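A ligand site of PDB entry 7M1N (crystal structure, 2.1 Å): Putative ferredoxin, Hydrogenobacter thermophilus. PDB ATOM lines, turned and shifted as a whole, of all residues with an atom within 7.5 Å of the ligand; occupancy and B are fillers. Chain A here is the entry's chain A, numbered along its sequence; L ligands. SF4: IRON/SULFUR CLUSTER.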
ATOM      1  N   MET A   6      -0.421 -19.986  35.148  1.00  0.00           N
ATOM      2  CA  MET A   6       0.357 -19.055  34.348  1.00  0.00           C
ATOM      3  C   MET A   6       1.189 -19.825  33.334  1.00  0.00           C
ATOM      4  O   MET A   6       1.327 -21.043  33.431  1.00  0.00           O
ATOM      5  CB  MET A   6       1.263 -18.184  35.232  1.00  0.00           C
ATOM      6  CG  MET A   6       2.407 -18.931  35.925  1.00  0.00           C
ATOM      7  SD  MET A   6       3.692 -17.797  36.503  1.00  0.00           S
ATOM      8  CE  MET A   6       4.731 -18.896  37.449  1.00  0.00           C
ATOM      9  N   VAL A   7       1.741 -19.103  32.356  1.00  0.00           N
ATOM     10  CA  VAL A   7       2.672 -19.682  31.392  1.00  0.00           C
ATOM     11  C   VAL A   7       4.012 -18.971  31.509  1.00  0.00           C
ATOM     12  O   VAL A   7       4.083 -17.750  31.575  1.00  0.00           O
ATOM     13  CB  VAL A   7       2.145 -19.562  29.941  1.00  0.00           C
ATOM     14  CG1 VAL A   7       3.194 -20.018  28.938  1.00  0.00           C
ATOM     15  CG2 VAL A   7       0.871 -20.375  29.786  1.00  0.00           C
ATOM     16  N   ASP A   8       5.076 -19.767  31.549  1.00  0.00           N
ATOM     17  CA  ASP A   8       6.429 -19.228  31.528  1.00  0.00           C
ATOM     18  C   ASP A   8       6.862 -19.070  30.059  1.00  0.00           C
ATOM     19  O   ASP A   8       7.152 -20.057  29.396  1.00  0.00           O
ATOM     20  CB  ASP A   8       7.398 -20.143  32.276  1.00  0.00           C
ATOM     21  CG  ASP A   8       8.730 -19.493  32.551  1.00  0.00           C
ATOM     22  OD1 ASP A   8       9.089 -18.523  31.843  1.00  0.00           O
ATOM     23  OD2 ASP A   8       9.433 -19.936  33.482  1.00  0.00           O
ATOM     24  N   PRO A   9       6.908 -17.821  29.562  1.00  0.00           N
ATOM     25  CA  PRO A   9       7.247 -17.643  28.150  1.00  0.00           C
ATOM     26  C   PRO A   9       8.688 -18.019  27.829  1.00  0.00           C
ATOM     27  O   PRO A   9       9.020 -18.276  26.679  1.00  0.00           O
ATOM     28  CB  PRO A   9       6.997 -16.154  27.916  1.00  0.00           C
ATOM     29  CG  PRO A   9       7.226 -15.531  29.248  1.00  0.00           C
ATOM     30  CD  PRO A   9       6.728 -16.532  30.249  1.00  0.00           C
ATOM     31  N   THR A  11      10.262 -20.655  28.465  1.00  0.00           N
ATOM     32  CA  THR A  11      10.454 -22.078  28.197  1.00  0.00           C
ATOM     33  C   THR A  11       9.444 -22.641  27.196  1.00  0.00           C
ATOM     34  O   THR A  11       9.617 -23.759  26.712  1.00  0.00           O
ATOM     35  CB  THR A  11      10.359 -22.898  29.493  1.00  0.00           C
ATOM     36  OG1 THR A  11       9.122 -22.600  30.160  1.00  0.00           O
ATOM     37  CG2 THR A  11      11.518 -22.574  30.418  1.00  0.00           C
ATOM     38  N   CYS A  12       8.407 -21.882  26.897  1.00  0.00           N
ATOM     39  CA  CYS A  12       7.379 -22.330  25.957  1.00  0.00           C
ATOM     40  C   CYS A  12       7.964 -22.613  24.589  1.00  0.00           C
ATOM     41  O   CYS A  12       8.729 -21.796  24.048  1.00  0.00           O
ATOM     42  CB  CYS A  12       6.260 -21.295  25.847  1.00  0.00           C
ATOM     43  SG  CYS A  12       4.977 -21.726  24.630  1.00  0.00           S
ATOM     44  N   THR A  13       7.619 -23.761  24.024  1.00  0.00           N
ATOM     45  CA  THR A  13       8.122 -24.182  22.720  1.00  0.00           C
ATOM     46  C   THR A  13       7.075 -24.011  21.622  1.00  0.00           C
ATOM     47  O   THR A  13       7.247 -24.490  20.500  1.00  0.00           O
ATOM     48  CB  THR A  13       8.592 -25.650  22.753  1.00  0.00           C
ATOM     49  OG1 THR A  13       7.514 -26.493  23.177  1.00  0.00           O
ATOM     50  CG2 THR A  13       9.763 -25.823  23.711  1.00  0.00           C
ATOM     51  N   SER A  14       5.986 -23.324  21.947  1.00  0.00           N
ATOM     52  CA  SER A  14       4.949 -22.984  20.976  1.00  0.00           C
ATOM     53  C   SER A  14       4.348 -24.211  20.305  1.00  0.00           C
ATOM     54  O   SER A  14       4.139 -24.238  19.095  1.00  0.00           O
ATOM     55  CB  SER A  14       5.511 -22.038  19.908  1.00  0.00           C
ATOM     56  OG  SER A  14       6.035 -20.850  20.501  1.00  0.00           O
ATOM     57  N   CYS A  15       4.069 -25.241  21.104  1.00  0.00           N
ATOM     58  CA  CYS A  15       3.539 -26.486  20.567  1.00  0.00           C
ATOM     59  C   CYS A  15       2.031 -26.395  20.310  1.00  0.00           C
ATOM     60  O   CYS A  15       1.435 -27.306  19.726  1.00  0.00           O
ATOM     61  CB  CYS A  15       3.835 -27.639  21.522  1.00  0.00           C
ATOM     62  SG  CYS A  15       2.675 -27.757  22.899  1.00  0.00           S
ATOM     63  N   GLU A  16       1.432 -25.301  20.768  1.00  0.00           N
ATOM     64  CA  GLU A  16       0.028 -24.967  20.511  1.00  0.00           C
ATOM     65  C   GLU A  16      -0.975 -25.837  21.276  1.00  0.00           C
ATOM     66  O   GLU A  16      -2.186 -25.711  21.073  1.00  0.00           O
ATOM     67  CB  GLU A  16      -0.293 -25.052  19.014  1.00  0.00           C
ATOM     68  CG  GLU A  16       0.674 -24.287  18.115  1.00  0.00           C
ATOM     69  CD  GLU A  16       0.120 -24.032  16.715  1.00  0.00           C
ATOM     70  OE1 GLU A  16      -1.028 -24.445  16.445  1.00  0.00           O
ATOM     71  OE2 GLU A  16       0.830 -23.428  15.880  1.00  0.00           O
ATOM     72  N   LEU A  17      -0.496 -26.704  22.157  1.00  0.00           N
ATOM     73  CA  LEU A  17      -1.392 -27.639  22.844  1.00  0.00           C
ATOM     74  C   LEU A  17      -2.366 -26.938  23.791  1.00  0.00           C
ATOM     75  O   LEU A  17      -3.573 -27.175  23.727  1.00  0.00           O
ATOM     76  CB  LEU A  17      -0.591 -28.681  23.628  1.00  0.00           C
ATOM     77  CG  LEU A  17      -1.424 -29.721  24.378  1.00  0.00           C
ATOM     78  CD1 LEU A  17      -2.269 -30.547  23.415  1.00  0.00           C
ATOM     79  CD2 LEU A  17      -0.536 -30.628  25.216  1.00  0.00           C
ATOM     80  N   CYS A  18      -1.857 -26.070  24.660  1.00  0.00           N
ATOM     81  CA  CYS A  18      -2.676 -25.496  25.715  1.00  0.00           C
ATOM     82  C   CYS A  18      -3.791 -24.582  25.205  1.00  0.00           C
ATOM     83  O   CYS A  18      -4.919 -24.668  25.680  1.00  0.00           O
ATOM     84  CB  CYS A  18      -1.810 -24.731  26.712  1.00  0.00           C
ATOM     85  SG  CYS A  18      -0.779 -23.438  25.997  1.00  0.00           S
ATOM     86  N   TYR A  19      -3.483 -23.714  24.243  1.00  0.00           N
ATOM     87  CA  TYR A  19      -4.502 -22.774  23.765  1.00  0.00           C
ATOM     88  C   TYR A  19      -5.339 -23.355  22.636  1.00  0.00           C
ATOM     89  O   TYR A  19      -6.309 -22.729  22.193  1.00  0.00           O
ATOM     90  CB  TYR A  19      -3.879 -21.438  23.320  1.00  0.00           C
ATOM     91  CG  TYR A  19      -2.677 -21.482  22.403  1.00  0.00           C
ATOM     92  CD1 TYR A  19      -1.409 -21.206  22.884  1.00  0.00           C
ATOM     93  CD2 TYR A  19      -2.823 -21.757  21.047  1.00  0.00           C
ATOM     94  CE1 TYR A  19      -0.308 -21.219  22.057  1.00  0.00           C
ATOM     95  CE2 TYR A  19      -1.720 -21.772  20.207  1.00  0.00           C
ATOM     96  CZ  TYR A  19      -0.469 -21.497  20.720  1.00  0.00           C
ATOM     97  OH  TYR A  19       0.640 -21.503  19.902  1.00  0.00           O
ATOM     98  N   ASP A  20      -5.003 -24.552  22.183  1.00  0.00           N
ATOM     99  CA  ASP A  20      -5.870 -25.292  21.286  1.00  0.00           C
ATOM    100  C   ASP A  20      -6.887 -26.108  22.077  1.00  0.00           C
ATOM    101  O   ASP A  20      -8.044 -26.241  21.677  1.00  0.00           O
ATOM    102  CB  ASP A  20      -5.068 -26.220  20.372  1.00  0.00           C
ATOM    103  CG  ASP A  20      -5.950 -27.026  19.442  1.00  0.00           C
ATOM    104  OD1 ASP A  20      -6.427 -26.464  18.445  1.00  0.00           O
ATOM    105  OD2 ASP A  20      -6.161 -28.229  19.722  1.00  0.00           O
ATOM    106  N   TYR A  26      -6.021 -20.292  27.878  1.00  0.00           N
ATOM    107  CA  TYR A  26      -4.775 -19.957  27.202  1.00  0.00           C
ATOM    108  C   TYR A  26      -5.013 -19.449  25.775  1.00  0.00           C
ATOM    109  O   TYR A  26      -6.005 -19.803  25.146  1.00  0.00           O
ATOM    110  CB  TYR A  26      -3.855 -21.180  27.159  1.00  0.00           C
ATOM    111  CG  TYR A  26      -3.678 -21.849  28.504  1.00  0.00           C
ATOM    112  CD1 TYR A  26      -2.766 -21.352  29.426  1.00  0.00           C
ATOM    113  CD2 TYR A  26      -4.412 -22.967  28.847  1.00  0.00           C
ATOM    114  CE1 TYR A  26      -2.602 -21.953  30.665  1.00  0.00           C
ATOM    115  CE2 TYR A  26      -4.255 -23.583  30.072  1.00  0.00           C
ATOM    116  CZ  TYR A  26      -3.350 -23.073  30.977  1.00  0.00           C
ATOM    117  OH  TYR A  26      -3.193 -23.675  32.200  1.00  0.00           O
ATOM    118  N   LYS A  27      -4.088 -18.622  25.298  1.00  0.00           N
ATOM    119  CA  LYS A  27      -4.144 -18.121  23.927  1.00  0.00           C
ATOM    120  C   LYS A  27      -2.748 -17.974  23.322  1.00  0.00           C
ATOM    121  O   LYS A  27      -1.765 -17.831  24.040  1.00  0.00           O
ATOM    122  CB  LYS A  27      -4.873 -16.764  23.880  1.00  0.00           C
ATOM    123  CG  LYS A  27      -4.174 -15.666  24.683  1.00  0.00           C
ATOM    124  CD  LYS A  27      -4.918 -14.340  24.606  1.00  0.00           C
ATOM    125  CE  LYS A  27      -4.152 -13.233  25.343  1.00  0.00           C
ATOM    126  NZ  LYS A  27      -4.893 -11.935  25.336  1.00  0.00           N
ATOM    127  N   GLY A  32       3.274 -17.482  18.595  1.00  0.00           N
ATOM    128  CA  GLY A  32       3.303 -18.910  18.860  1.00  0.00           C
ATOM    129  C   GLY A  32       3.423 -19.239  20.348  1.00  0.00           C
ATOM    130  O   GLY A  32       3.032 -20.322  20.771  1.00  0.00           O
ATOM    131  N   ILE A  33       3.978 -18.313  21.118  1.00  0.00           N
ATOM    132  CA  ILE A  33       4.124 -18.514  22.560  1.00  0.00           C
ATOM    133  C   ILE A  33       2.770 -18.405  23.254  1.00  0.00           C
ATOM    134  O   ILE A  33       1.966 -17.519  22.947  1.00  0.00           O
ATOM    135  CB  ILE A  33       5.094 -17.488  23.192  1.00  0.00           C
ATOM    136  CG1 ILE A  33       6.501 -17.653  22.612  1.00  0.00           C
ATOM    137  CG2 ILE A  33       5.122 -17.615  24.715  1.00  0.00           C
ATOM    138  CD1 ILE A  33       7.182 -18.966  22.971  1.00  0.00           C
ATOM    139  N   ALA A  34       2.524 -19.307  24.205  1.00  0.00           N
ATOM    140  CA  ALA A  34       1.259 -19.329  24.933  1.00  0.00           C
ATOM    141  C   ALA A  34       1.240 -18.284  26.043  1.00  0.00           C
ATOM    142  O   ALA A  34       2.275 -17.901  26.576  1.00  0.00           O
ATOM    143  CB  ALA A  34       1.005 -20.704  25.509  1.00  0.00           C
ATOM    144  N   GLU A  35       0.034 -17.838  26.379  1.00  0.00           N
ATOM    145  CA  GLU A  35      -0.175 -16.863  27.448  1.00  0.00           C
ATOM    146  C   GLU A  35      -1.587 -17.023  27.985  1.00  0.00           C
ATOM    147  O   GLU A  35      -2.514 -17.311  27.217  1.00  0.00           O
ATOM    148  CB  GLU A  35       0.055 -15.443  26.941  1.00  0.00           C
ATOM    149  CG  GLU A  35      -0.172 -14.356  27.978  1.00  0.00           C
ATOM    150  CD  GLU A  35       0.022 -12.962  27.401  1.00  0.00           C
ATOM    151  OE1 GLU A  35       0.359 -12.854  26.209  1.00  0.00           O
ATOM    152  OE2 GLU A  35      -0.176 -11.979  28.151  1.00  0.00           O
ATOM    153  N   VAL A  58      -3.557 -30.169  30.931  1.00  0.00           N
ATOM    154  CA  VAL A  58      -2.604 -29.539  30.023  1.00  0.00           C
ATOM    155  C   VAL A  58      -1.328 -29.157  30.763  1.00  0.00           C
ATOM    156  O   VAL A  58      -0.255 -29.094  30.162  1.00  0.00           O
ATOM    157  CB  VAL A  58      -3.192 -28.288  29.334  1.00  0.00           C
ATOM    158  CG1 VAL A  58      -4.363 -28.670  28.450  1.00  0.00           C
ATOM    159  CG2 VAL A  58      -3.602 -27.240  30.357  1.00  0.00           C
ATOM    160  N   THR A  59      -1.445 -28.892  32.055  1.00  0.00           N
ATOM    161  CA  THR A  59      -0.275 -28.616  32.878  1.00  0.00           C
ATOM    162  C   THR A  59       0.666 -29.820  32.882  1.00  0.00           C
ATOM    163  O   THR A  59       1.885 -29.672  32.784  1.00  0.00           O
ATOM    164  CB  THR A  59      -0.670 -28.258  34.330  1.00  0.00           C
ATOM    165  OG1 THR A  59      -1.481 -27.082  34.337  1.00  0.00           O
ATOM    166  CG2 THR A  59       0.573 -28.011  35.188  1.00  0.00           C
ATOM    167  N   GLU A  61       0.553 -32.158  30.563  1.00  0.00           N
ATOM    168  CA  GLU A  61       0.790 -32.534  29.173  1.00  0.00           C
ATOM    169  C   GLU A  61       1.744 -31.592  28.455  1.00  0.00           C
ATOM    170  O   GLU A  61       2.319 -31.945  27.436  1.00  0.00           O
ATOM    171  CB  GLU A  61      -0.532 -32.607  28.423  1.00  0.00           C
ATOM    172  CG  GLU A  61      -1.363 -33.840  28.766  1.00  0.00           C
ATOM    173  CD  GLU A  61      -2.780 -33.769  28.240  1.00  0.00           C
ATOM    174  OE1 GLU A  61      -3.203 -32.690  27.783  1.00  0.00           O
ATOM    175  OE2 GLU A  61      -3.472 -34.807  28.277  1.00  0.00           O
ATOM    176  N   CYS A  62       1.895 -30.378  28.984  1.00  0.00           N
ATOM    177  CA  CYS A  62       2.810 -29.405  28.399  1.00  0.00           C
ATOM    178  C   CYS A  62       4.210 -30.003  28.307  1.00  0.00           C
ATOM    179  O   CYS A  62       4.784 -30.378  29.325  1.00  0.00           O
ATOM    180  CB  CYS A  62       2.824 -28.122  29.225  1.00  0.00           C
ATOM    181  SG  CYS A  62       4.111 -26.946  28.720  1.00  0.00           S
ATOM    182  N   PRO A  63       4.771 -30.085  27.085  1.00  0.00           N
ATOM    183  CA  PRO A  63       6.065 -30.778  26.900  1.00  0.00           C
ATOM    184  C   PRO A  63       7.247 -30.058  27.535  1.00  0.00           C
ATOM    185  O   PRO A  63       8.267 -30.700  27.795  1.00  0.00           O
ATOM    186  CB  PRO A  63       6.213 -30.812  25.384  1.00  0.00           C
ATOM    187  CG  PRO A  63       5.443 -29.649  24.891  1.00  0.00           C
ATOM    188  CD  PRO A  63       4.253 -29.555  25.812  1.00  0.00           C
ATOM    189  N   SER A  64       7.125 -28.755  27.789  1.00  0.00           N
ATOM    190  CA  SER A  64       8.251 -27.945  28.233  1.00  0.00           C
ATOM    191  C   SER A  64       8.150 -27.541  29.708  1.00  0.00           C
ATOM    192  O   SER A  64       9.003 -26.813  30.210  1.00  0.00           O
ATOM    193  CB  SER A  64       8.371 -26.690  27.365  1.00  0.00           C
ATOM    194  OG  SER A  64       7.181 -25.925  27.425  1.00  0.00           O
ATOM    195  N   GLY A  65       7.101 -28.010  30.392  1.00  0.00           N
ATOM    196  CA  GLY A  65       6.894 -27.657  31.784  1.00  0.00           C
ATOM    197  C   GLY A  65       6.714 -26.157  31.972  1.00  0.00           C
ATOM    198  O   GLY A  65       7.021 -25.617  33.033  1.00  0.00           O
ATOM    199  N   SER A  66       6.198 -25.495  30.940  1.00  0.00           N
ATOM    200  CA  SER A  66       6.067 -24.039  30.947  1.00  0.00           C
ATOM    201  C   SER A  66       4.830 -23.561  31.695  1.00  0.00           C
ATOM    202  O   SER A  66       4.746 -22.407  32.114  1.00  0.00           O
ATOM    203  CB  SER A  66       6.035 -23.502  29.519  1.00  0.00           C
ATOM    204  OG  SER A  66       7.244 -23.793  28.838  1.00  0.00           O
ATOM    205  N   ILE A  67       3.854 -24.455  31.841  1.00  0.00           N
ATOM    206  CA  ILE A  67       2.606 -24.105  32.522  1.00  0.00           C
ATOM    207  C   ILE A  67       2.727 -24.377  34.018  1.00  0.00           C
ATOM    208  O   ILE A  67       2.983 -25.506  34.429  1.00  0.00           O
ATOM    209  CB  ILE A  67       1.407 -24.880  31.956  1.00  0.00           C
ATOM    210  CG1 ILE A  67       1.257 -24.585  30.458  1.00  0.00           C
ATOM    211  CG2 ILE A  67       0.124 -24.513  32.707  1.00  0.00           C
ATOM    212  CD1 ILE A  67       0.126 -25.335  29.773  1.00  0.00           C
HETATM  213 FE1  SF4 L   1       3.889 -23.625  25.245  1.00  0.00          FE
HETATM  214 FE2  SF4 L   1       3.394 -25.690  26.973  1.00  0.00          FE
HETATM  215 FE3  SF4 L   1       2.865 -25.982  24.317  1.00  0.00          FE
HETATM  216 FE4  SF4 L   1       1.313 -24.319  25.830  1.00  0.00          FE
HETATM  217  S1  SF4 L   1       1.511 -26.569  26.049  1.00  0.00           S
HETATM  218  S2  SF4 L   1       2.180 -23.875  23.773  1.00  0.00           S
HETATM  219  S3  SF4 L   1       2.868 -23.490  27.285  1.00  0.00           S
HETATM  220  S4  SF4 L   1       4.909 -25.659  25.278  1.00  0.00           S
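FE2 of the ligand is bound by SG of Cys 62, at 2.3 Å. An iron atom (FE1) of the ligand is bound by the side-chain sulfur (SG) of Cys 12. The backbone NH (N) of Cys 18 sits close to a sulfur (S1) of the ligand (3.7 Å). SG of Cys 18 binds FE4 of the ligand. The backbone NH (N) of Cys 15 lies close to a sulfur (S2) of the ligand (3.5 Å). SG of Cys 15 is bound to FE3 of the ligand. S4 of the ligand sits close to OG of Ser 64. The backbone NH (N) of Glu 16 sits close to a sulfur (S2) of the ligand. The backbone NH (N) of Thr 13 sits close to a sulfur (S4) of the ligand (3.5 Å). The side-chain hydroxyl of Thr 13 lies close to a sulfur (S4) of the ligand (3.4 Å).
The side-chain hydroxyl (OG) of Ser 64 lies close to the side-chain sulfur (SG) of Cys 62 (3.5 Å). The side-chain sulfur (SG) of Cys 62 sits close to the backbone NH (N) of Gly 65. SG of Cys 12 lies close to N of Ala 34 (3.5 Å). N of Cys 12 is in hydrogen-bond range of OG of Ser 66. The side-chain sulfur (SG) of Cys 12 sits close to the backbone NH (N) of Ser 14, 3.3 Å away. The backbone NH (N) of Leu 17 sits close to the side-chain sulfur (SG) of Cys 15 (3.4 Å). OG of Ser 64 sits at hydrogen-bond distance from OG of Ser 66 (2.6 Å). OG of Ser 66 lies within hydrogen-bond range of OG1 of Thr 11 (2.6 Å).
Val 7 touches the ligand (CG1 to S3, 3.9 Å). Ser 14 touches the ligand. CB of Leu 17 touches S1 of the ligand (3.8 Å). Ala 34 touches the ligand (CB to FE4, 3.6 Å). Pro 63 touches the ligand (CD to S4, 3.99 Å). CB of Ser 66 touches S3 of the ligand, 3.9 Å away. Ile 67 touches the ligand (CG1 to S3, 3.7 Å). Hydrophobic or aromatic side chains that line the ligand: Val 7, Leu 17, Ala 34, Pro 63 and Ile 67. Of the 29 residues printed, 14 come within 4 Å of the ligand. Along chain A the residues within 4 Å of the ligand span positions 7 to 67.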
